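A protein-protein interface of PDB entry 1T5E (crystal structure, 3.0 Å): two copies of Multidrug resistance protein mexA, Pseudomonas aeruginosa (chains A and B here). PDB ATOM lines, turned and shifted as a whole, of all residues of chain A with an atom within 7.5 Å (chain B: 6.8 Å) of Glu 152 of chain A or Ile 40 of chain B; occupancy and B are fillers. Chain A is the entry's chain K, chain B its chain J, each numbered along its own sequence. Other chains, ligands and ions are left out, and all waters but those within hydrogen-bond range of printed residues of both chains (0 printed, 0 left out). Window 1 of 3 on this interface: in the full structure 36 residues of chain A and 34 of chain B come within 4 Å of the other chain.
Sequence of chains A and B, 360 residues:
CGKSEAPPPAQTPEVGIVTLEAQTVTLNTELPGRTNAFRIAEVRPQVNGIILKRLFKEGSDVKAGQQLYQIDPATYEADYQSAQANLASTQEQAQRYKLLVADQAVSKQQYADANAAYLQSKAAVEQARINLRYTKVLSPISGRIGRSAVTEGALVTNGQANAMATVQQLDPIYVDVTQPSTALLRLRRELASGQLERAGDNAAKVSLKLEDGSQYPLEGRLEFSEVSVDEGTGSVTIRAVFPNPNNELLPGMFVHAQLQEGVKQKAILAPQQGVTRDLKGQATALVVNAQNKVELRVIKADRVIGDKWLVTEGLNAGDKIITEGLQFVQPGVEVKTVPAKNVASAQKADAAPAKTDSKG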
ATOM      1  N   ILE A  50      12.876  24.481  33.367  1.00  0.00           N
ATOM      2  CA  ILE A  50      12.794  24.912  31.966  1.00  0.00           C
ATOM      3  C   ILE A  50      12.015  23.909  31.109  1.00  0.00           C
ATOM      4  O   ILE A  50      12.259  22.684  31.184  1.00  0.00           O
ATOM      5  CB  ILE A  50      14.199  25.065  31.308  1.00  0.00           C
ATOM      6  CG1 ILE A  50      14.976  26.222  31.937  1.00  0.00           C
ATOM      7  CG2 ILE A  50      14.012  25.390  29.836  1.00  0.00           C
ATOM      8  CD1 ILE A  50      14.243  27.598  31.735  1.00  0.00           C
ATOM      9  N   ILE A  51      11.080  24.416  30.308  1.00  0.00           N
ATOM     10  CA  ILE A  51      10.312  23.551  29.398  1.00  0.00           C
ATOM     11  C   ILE A  51      11.272  22.974  28.330  1.00  0.00           C
ATOM     12  O   ILE A  51      11.791  23.720  27.498  1.00  0.00           O
ATOM     13  CB  ILE A  51       9.225  24.350  28.626  1.00  0.00           C
ATOM     14  CG1 ILE A  51       8.204  24.955  29.594  1.00  0.00           C
ATOM     15  CG2 ILE A  51       8.543  23.453  27.621  1.00  0.00           C
ATOM     16  CD1 ILE A  51       7.328  23.925  30.308  1.00  0.00           C
ATOM     17  N   LEU A  52      11.531  21.670  28.360  1.00  0.00           N
ATOM     18  CA  LEU A  52      12.416  21.041  27.368  1.00  0.00           C
ATOM     19  C   LEU A  52      11.599  20.800  26.099  1.00  0.00           C
ATOM     20  O   LEU A  52      11.940  21.279  25.026  1.00  0.00           O
ATOM     21  CB  LEU A  52      12.912  19.700  27.866  1.00  0.00           C
ATOM     22  CG  LEU A  52      14.373  19.366  27.665  1.00  0.00           C
ATOM     23  CD1 LEU A  52      15.178  20.536  28.089  1.00  0.00           C
ATOM     24  CD2 LEU A  52      14.780  18.158  28.505  1.00  0.00           C
ATOM     25  N   LYS A  53      10.498  20.073  26.222  1.00  0.00           N
ATOM     26  CA  LYS A  53       9.672  19.786  25.065  1.00  0.00           C
ATOM     27  C   LYS A  53       8.194  19.948  25.313  1.00  0.00           C
ATOM     28  O   LYS A  53       7.706  19.777  26.434  1.00  0.00           O
ATOM     29  CB  LYS A  53       9.955  18.363  24.567  1.00  0.00           C
ATOM     30  CG  LYS A  53      11.309  18.255  23.888  1.00  0.00           C
ATOM     31  CD  LYS A  53      11.751  16.828  23.572  1.00  0.00           C
ATOM     32  CE  LYS A  53      13.159  16.850  22.905  1.00  0.00           C
ATOM     33  NZ  LYS A  53      13.698  15.487  22.532  1.00  0.00           N
ATOM     34  N   ARG A  54       7.476  20.284  24.256  1.00  0.00           N
ATOM     35  CA  ARG A  54       6.044  20.421  24.339  1.00  0.00           C
ATOM     36  C   ARG A  54       5.396  19.341  23.454  1.00  0.00           C
ATOM     37  O   ARG A  54       5.007  19.628  22.335  1.00  0.00           O
ATOM     38  CB  ARG A  54       5.633  21.797  23.858  1.00  0.00           C
ATOM     39  CG  ARG A  54       4.140  22.004  23.923  1.00  0.00           C
ATOM     40  CD  ARG A  54       3.550  21.987  22.582  1.00  0.00           C
ATOM     41  NE  ARG A  54       3.666  23.287  21.948  1.00  0.00           N
ATOM     42  CZ  ARG A  54       3.341  23.490  20.679  1.00  0.00           C
ATOM     43  NH1 ARG A  54       2.899  22.475  19.950  1.00  0.00           N
ATOM     44  NH2 ARG A  54       3.439  24.693  20.142  1.00  0.00           N
ATOM     45  N   LEU A  55       5.266  18.121  23.981  1.00  0.00           N
ATOM     46  CA  LEU A  55       4.703  16.964  23.300  1.00  0.00           C
ATOM     47  C   LEU A  55       3.232  16.949  22.826  1.00  0.00           C
ATOM     48  O   LEU A  55       2.552  15.934  22.995  1.00  0.00           O
ATOM     49  CB  LEU A  55       4.899  15.737  24.178  1.00  0.00           C
ATOM     50  CG  LEU A  55       6.133  15.772  25.075  1.00  0.00           C
ATOM     51  CD1 LEU A  55       6.379  14.428  25.743  1.00  0.00           C
ATOM     52  CD2 LEU A  55       7.336  16.147  24.232  1.00  0.00           C
ATOM     53  N   TYR A  69       3.972  17.970  28.469  1.00  0.00           N
ATOM     54  CA  TYR A  69       5.221  18.726  28.537  1.00  0.00           C
ATOM     55  C   TYR A  69       6.289  17.980  29.259  1.00  0.00           C
ATOM     56  O   TYR A  69       6.013  17.104  30.062  1.00  0.00           O
ATOM     57  CB  TYR A  69       5.058  20.005  29.328  1.00  0.00           C
ATOM     58  CG  TYR A  69       4.180  21.044  28.699  1.00  0.00           C
ATOM     59  CD1 TYR A  69       2.838  21.100  29.002  1.00  0.00           C
ATOM     60  CD2 TYR A  69       4.696  21.988  27.815  1.00  0.00           C
ATOM     61  CE1 TYR A  69       2.024  22.065  28.462  1.00  0.00           C
ATOM     62  CE2 TYR A  69       3.873  22.973  27.256  1.00  0.00           C
ATOM     63  CZ  TYR A  69       2.539  23.003  27.590  1.00  0.00           C
ATOM     64  OH  TYR A  69       1.695  23.965  27.075  1.00  0.00           O
ATOM     65  N   SER A 148      -0.607  26.529  23.241  1.00  0.00           N
ATOM     66  CA  SER A 148       0.181  26.353  24.455  1.00  0.00           C
ATOM     67  C   SER A 148       0.644  27.732  24.846  1.00  0.00           C
ATOM     68  O   SER A 148       1.449  28.318  24.137  1.00  0.00           O
ATOM     69  CB  SER A 148       1.406  25.503  24.192  1.00  0.00           C
ATOM     70  OG  SER A 148       2.358  25.696  25.220  1.00  0.00           O
ATOM     71  N   VAL A 150       2.701  28.568  26.811  1.00  0.00           N
ATOM     72  CA  VAL A 150       4.107  28.577  27.174  1.00  0.00           C
ATOM     73  C   VAL A 150       4.986  28.046  26.019  1.00  0.00           C
ATOM     74  O   VAL A 150       4.690  26.992  25.453  1.00  0.00           O
ATOM     75  CB  VAL A 150       4.289  27.747  28.463  1.00  0.00           C
ATOM     76  CG1 VAL A 150       5.612  27.033  28.495  1.00  0.00           C
ATOM     77  CG2 VAL A 150       4.197  28.672  29.637  1.00  0.00           C
ATOM     78  N   THR A 151       6.049  28.770  25.664  1.00  0.00           N
ATOM     79  CA  THR A 151       6.929  28.341  24.579  1.00  0.00           C
ATOM     80  C   THR A 151       7.903  27.333  25.129  1.00  0.00           C
ATOM     81  O   THR A 151       7.997  27.171  26.330  1.00  0.00           O
ATOM     82  CB  THR A 151       7.764  29.495  24.012  1.00  0.00           C
ATOM     83  OG1 THR A 151       8.792  29.841  24.949  1.00  0.00           O
ATOM     84  CG2 THR A 151       6.894  30.711  23.724  1.00  0.00           C
ATOM     85  N   GLU A 152       8.634  26.642  24.263  1.00  0.00           N
ATOM     86  CA  GLU A 152       9.612  25.668  24.752  1.00  0.00           C
ATOM     87  C   GLU A 152      10.735  26.527  25.305  1.00  0.00           C
ATOM     88  O   GLU A 152      10.808  27.737  25.022  1.00  0.00           O
ATOM     89  CB  GLU A 152      10.115  24.768  23.609  1.00  0.00           C
ATOM     90  CG  GLU A 152       9.061  24.562  22.496  1.00  0.00           C
ATOM     91  CD  GLU A 152       9.239  23.260  21.685  1.00  0.00           C
ATOM     92  OE1 GLU A 152       8.532  23.109  20.654  1.00  0.00           O
ATOM     93  OE2 GLU A 152      10.064  22.389  22.069  1.00  0.00           O
ATOM     94  N   GLY A 153      11.589  25.925  26.113  1.00  0.00           N
ATOM     95  CA  GLY A 153      12.689  26.679  26.673  1.00  0.00           C
ATOM     96  C   GLY A 153      12.294  27.749  27.683  1.00  0.00           C
ATOM     97  O   GLY A 153      13.166  28.374  28.290  1.00  0.00           O
ATOM     98  N   ALA A 154      10.992  27.973  27.858  1.00  0.00           N
ATOM     99  CA  ALA A 154      10.484  28.954  28.822  1.00  0.00           C
ATOM    100  C   ALA A 154      10.688  28.524  30.294  1.00  0.00           C
ATOM    101  O   ALA A 154      10.830  27.320  30.613  1.00  0.00           O
ATOM    102  CB  ALA A 154       9.014  29.210  28.568  1.00  0.00           C
ATOM    103  N   LEU A 155      10.732  29.524  31.179  1.00  0.00           N
ATOM    104  CA  LEU A 155      10.906  29.277  32.606  1.00  0.00           C
ATOM    105  C   LEU A 155       9.528  29.035  33.193  1.00  0.00           C
ATOM    106  O   LEU A 155       8.585  29.806  32.947  1.00  0.00           O
ATOM    107  CB  LEU A 155      11.534  30.474  33.303  1.00  0.00           C
ATOM    108  CG  LEU A 155      11.788  30.206  34.787  1.00  0.00           C
ATOM    109  CD1 LEU A 155      12.739  29.012  34.964  1.00  0.00           C
ATOM    110  CD2 LEU A 155      12.379  31.433  35.405  1.00  0.00           C
ATOM    111  N   ASN B  36       1.865  34.431  11.832  1.00  0.00           N
ATOM    112  CA  ASN B  36       2.476  34.116  13.117  1.00  0.00           C
ATOM    113  C   ASN B  36       3.575  33.091  12.963  1.00  0.00           C
ATOM    114  O   ASN B  36       3.515  32.221  12.102  1.00  0.00           O
ATOM    115  CB  ASN B  36       1.438  33.581  14.125  1.00  0.00           C
ATOM    116  CG  ASN B  36       0.518  34.682  14.673  1.00  0.00           C
ATOM    117  OD1 ASN B  36       0.987  35.715  15.208  1.00  0.00           O
ATOM    118  ND2 ASN B  36      -0.798  34.468  14.550  1.00  0.00           N
ATOM    119  N   ALA B  37       4.584  33.191  13.810  1.00  0.00           N
ATOM    120  CA  ALA B  37       5.686  32.262  13.737  1.00  0.00           C
ATOM    121  C   ALA B  37       5.115  30.874  13.788  1.00  0.00           C
ATOM    122  O   ALA B  37       4.078  30.632  14.375  1.00  0.00           O
ATOM    123  CB  ALA B  37       6.629  32.479  14.887  1.00  0.00           C
ATOM    124  N   PHE B  38       5.810  29.957  13.160  1.00  0.00           N
ATOM    125  CA  PHE B  38       5.397  28.562  13.117  1.00  0.00           C
ATOM    126  C   PHE B  38       5.718  27.889  14.446  1.00  0.00           C
ATOM    127  O   PHE B  38       5.041  26.942  14.850  1.00  0.00           O
ATOM    128  CB  PHE B  38       6.185  27.846  12.012  1.00  0.00           C
ATOM    129  CG  PHE B  38       5.668  26.486  11.675  1.00  0.00           C
ATOM    130  CD1 PHE B  38       4.407  26.337  11.045  1.00  0.00           C
ATOM    131  CD2 PHE B  38       6.445  25.363  11.937  1.00  0.00           C
ATOM    132  CE1 PHE B  38       3.952  25.085  10.685  1.00  0.00           C
ATOM    133  CE2 PHE B  38       5.990  24.089  11.580  1.00  0.00           C
ATOM    134  CZ  PHE B  38       4.744  23.949  10.954  1.00  0.00           C
ATOM    135  N   ARG B  39       6.775  28.375  15.098  1.00  0.00           N
ATOM    136  CA  ARG B  39       7.232  27.797  16.355  1.00  0.00           C
ATOM    137  C   ARG B  39       8.159  28.757  17.092  1.00  0.00           C
ATOM    138  O   ARG B  39       9.039  29.361  16.478  1.00  0.00           O
ATOM    139  CB  ARG B  39       7.946  26.500  16.055  1.00  0.00           C
ATOM    140  CG  ARG B  39       8.243  25.665  17.228  1.00  0.00           C
ATOM    141  CD  ARG B  39       8.743  24.325  16.732  1.00  0.00           C
ATOM    142  NE  ARG B  39       9.376  23.498  17.765  1.00  0.00           N
ATOM    143  CZ  ARG B  39      10.055  22.377  17.494  1.00  0.00           C
ATOM    144  NH1 ARG B  39      10.180  21.967  16.230  1.00  0.00           N
ATOM    145  NH2 ARG B  39      10.606  21.660  18.472  1.00  0.00           N
ATOM    146  N   ILE B  40       7.958  28.902  18.407  1.00  0.00           N
ATOM    147  CA  ILE B  40       8.779  29.809  19.213  1.00  0.00           C
ATOM    148  C   ILE B  40       9.416  29.149  20.424  1.00  0.00           C
ATOM    149  O   ILE B  40       8.823  28.255  21.031  1.00  0.00           O
ATOM    150  CB  ILE B  40       7.952  30.980  19.673  1.00  0.00           C
ATOM    151  CG1 ILE B  40       7.180  31.515  18.478  1.00  0.00           C
ATOM    152  CG2 ILE B  40       8.846  32.054  20.264  1.00  0.00           C
ATOM    153  CD1 ILE B  40       6.546  32.812  18.718  1.00  0.00           C
ATOM    154  N   ALA B  41      10.639  29.563  20.745  1.00  0.00           N
ATOM    155  CA  ALA B  41      11.358  29.021  21.891  1.00  0.00           C
ATOM    156  C   ALA B  41      12.111  30.180  22.524  1.00  0.00           C
ATOM    157  O   ALA B  41      12.298  31.215  21.869  1.00  0.00           O
ATOM    158  CB  ALA B  41      12.320  27.933  21.467  1.00  0.00           C
ATOM    159  N   GLU B  42      12.511  30.018  23.790  1.00  0.00           N
ATOM    160  CA  GLU B  42      13.232  31.052  24.515  1.00  0.00           C
ATOM    161  C   GLU B  42      14.569  30.493  24.936  1.00  0.00           C
ATOM    162  O   GLU B  42      14.684  29.300  25.226  1.00  0.00           O
ATOM    163  CB  GLU B  42      12.467  31.460  25.776  1.00  0.00           C
ATOM    164  CG  GLU B  42      11.278  32.417  25.594  1.00  0.00           C
ATOM    165  CD  GLU B  42      10.477  32.623  26.908  1.00  0.00           C
ATOM    166  OE1 GLU B  42      11.015  32.336  28.015  1.00  0.00           O
ATOM    167  OE2 GLU B  42       9.309  33.084  26.827  1.00  0.00           O
ATOM    168  N   VAL B  43      15.581  31.352  24.996  1.00  0.00           N
ATOM    169  CA  VAL B  43      16.907  30.918  25.408  1.00  0.00           C
ATOM    170  C   VAL B  43      17.114  31.447  26.837  1.00  0.00           C
ATOM    171  O   VAL B  43      16.944  32.650  27.086  1.00  0.00           O
ATOM    172  CB  VAL B  43      17.974  31.487  24.457  1.00  0.00           C
ATOM    173  CG1 VAL B  43      19.279  30.724  24.612  1.00  0.00           C
ATOM    174  CG2 VAL B  43      17.484  31.415  23.046  1.00  0.00           C
ATOM    175  N   PRO B 140      17.161  25.664  21.733  1.00  0.00           N
ATOM    176  CA  PRO B 140      16.159  24.590  21.751  1.00  0.00           C
ATOM    177  C   PRO B 140      15.497  24.268  20.397  1.00  0.00           C
ATOM    178  O   PRO B 140      15.185  23.140  20.095  1.00  0.00           O
ATOM    179  CB  PRO B 140      15.130  25.117  22.755  1.00  0.00           C
ATOM    180  CG  PRO B 140      15.104  26.571  22.408  1.00  0.00           C
ATOM    181  CD  PRO B 140      16.603  26.901  22.313  1.00  0.00           C
ATOM    182  N   ILE B 141      15.294  25.277  19.586  1.00  0.00           N
ATOM    183  CA  ILE B 141      14.601  25.108  18.343  1.00  0.00           C
ATOM    184  C   ILE B 141      15.466  25.526  17.150  1.00  0.00           C
ATOM    185  O   ILE B 141      16.565  26.029  17.319  1.00  0.00           O
ATOM    186  CB  ILE B 141      13.281  25.947  18.478  1.00  0.00           C
ATOM    187  CG1 ILE B 141      12.122  24.994  18.675  1.00  0.00           C
ATOM    188  CG2 ILE B 141      13.075  26.902  17.362  1.00  0.00           C
ATOM    189  CD1 ILE B 141      12.395  23.977  19.765  1.00  0.00           C
ATOM    190  N   THR B 166      15.182  35.043  21.888  1.00  0.00           N
ATOM    191  CA  THR B 166      14.085  34.256  21.334  1.00  0.00           C
ATOM    192  C   THR B 166      14.304  33.778  19.888  1.00  0.00           C
ATOM    193  O   THR B 166      14.426  34.595  18.970  1.00  0.00           O
ATOM    194  CB  THR B 166      12.829  35.088  21.318  1.00  0.00           C
ATOM    195  OG1 THR B 166      12.699  35.724  22.584  1.00  0.00           O
ATOM    196  CG2 THR B 166      11.608  34.230  21.018  1.00  0.00           C
ATOM    197  N   VAL B 167      14.326  32.466  19.689  1.00  0.00           N
ATOM    198  CA  VAL B 167      14.485  31.865  18.371  1.00  0.00           C
ATOM    199  C   VAL B 167      13.087  31.630  17.772  1.00  0.00           C
ATOM    200  O   VAL B 167      12.208  31.093  18.431  1.00  0.00           O
ATOM    201  CB  VAL B 167      15.180  30.509  18.505  1.00  0.00           C
ATOM    202  CG1 VAL B 167      15.239  29.822  17.176  1.00  0.00           C
ATOM    203  CG2 VAL B 167      16.559  30.673  19.105  1.00  0.00           C
ATOM    204  N   GLN B 168      12.845  32.038  16.539  1.00  0.00           N
ATOM    205  CA  GLN B 168      11.520  31.778  15.948  1.00  0.00           C
ATOM    206  C   GLN B 168      11.596  31.129  14.564  1.00  0.00           C
ATOM    207  O   GLN B 168      12.203  31.689  13.642  1.00  0.00           O
ATOM    208  CB  GLN B 168      10.714  33.045  15.772  1.00  0.00           C
ATOM    209  CG  GLN B 168      10.351  33.766  16.998  1.00  0.00           C
ATOM    210  CD  GLN B 168       9.297  34.777  16.664  1.00  0.00           C
ATOM    211  OE1 GLN B 168       9.213  35.234  15.533  1.00  0.00           O
ATOM    212  NE2 GLN B 168       8.481  35.128  17.626  1.00  0.00           N
ATOM    213  N   GLN B 169      10.977  29.962  14.414  1.00  0.00           N
ATOM    214  CA  GLN B 169      10.956  29.281  13.122  1.00  0.00           C
ATOM    215  C   GLN B 169       9.875  29.919  12.253  1.00  0.00           C
ATOM    216  O   GLN B 169       8.697  29.788  12.526  1.00  0.00           O
ATOM    217  CB  GLN B 169      10.691  27.805  13.325  1.00  0.00           C
ATOM    218  CG  GLN B 169      10.248  27.052  12.128  1.00  0.00           C
ATOM    219  CD  GLN B 169      10.049  25.596  12.475  1.00  0.00           C
ATOM    220  OE1 GLN B 169       9.260  24.893  11.844  1.00  0.00           O
ATOM    221  NE2 GLN B 169      10.775  25.125  13.500  1.00  0.00           N
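NE of Arg 39 of chain B lies within salt-bridge range of OE1 of Glu 152 of chain A, at 3.0 Å. The backbone NH (N) of Glu 42 of chain B sits at hydrogen-bond distance from the backbone carbonyl oxygen (O) of Glu 152 of chain A (3.1 Å).
The backbone carbonyl oxygen (O) of Ala 154 of chain A lies within hydrogen-bond range of the backbone NH (N) of Ile 51 of chain A, 2.9 Å away. O of Arg 39 of chain B is in hydrogen-bond range of N of Gln 169 of chain B, at 2.9 Å. The backbone NH (N) of Ala 41 of chain B is in hydrogen-bond range of the backbone carbonyl oxygen (O) of Val 167 of chain B (3.2 Å). The backbone NH of Gly 153 of chain A sits at hydrogen-bond distance from the backbone carbonyl oxygen of Ile 51 of chain A (2.6 Å).
Glu 152 of chain A touches five residues of chain B. Of the printed residues of chain B, Gly 153 of chain A touches Glu 42 (3.5 Å). Printed residues of chain B within 4 Å of Ala 154 of chain A: Glu 42. Of the printed residues of chain A, Arg 39 of chain B touches Glu 152 (3.0 Å). Of chain A, only Thr 151 (3.4 Å) and Glu 152 (3.6 Å) come within 4 Å of Ile 40 of chain B. Of the printed residues of chain A, Ile 141 of chain B touches Glu 152.
Hydrophobic or aromatic side chains of chain A that line the printed part of chain B: Ala 154. Of the 14 printed residues of chain B, 5 touch a printed residue of chain A. Hydrophobic or aromatic side chains of chain B within 4 Å of the printed part of chain A: Ala 41 and Ile 141. Among the printed residues, Asp or Glu carboxylates within 4 Å of a Lys or Arg side-chain nitrogen of the other chain: Glu 152 of chain A with Arg 39 of chain B.
Thr 151 of chain A touches Ile 40 of chain B. Glu 42 of chain B touches Thr 151 of chain A. Ile 40 of chain B touches Glu 152 of chain A. Glu 152 of chain A touches Ala 41 of chain B. Ile 141 of chain B touches Glu 152 of chain A. Gly 153 of chain A touches Glu 42 of chain B (O to O, 3.5 Å). CA of Ala 154 of chain A touches OE1 of Glu 42 of chain B, at 3.5 Å.
No position is printed for both chains. Of the 9 pairs that touch across the chains among the printed residues, none has its exchanged pair printed and touching as well.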
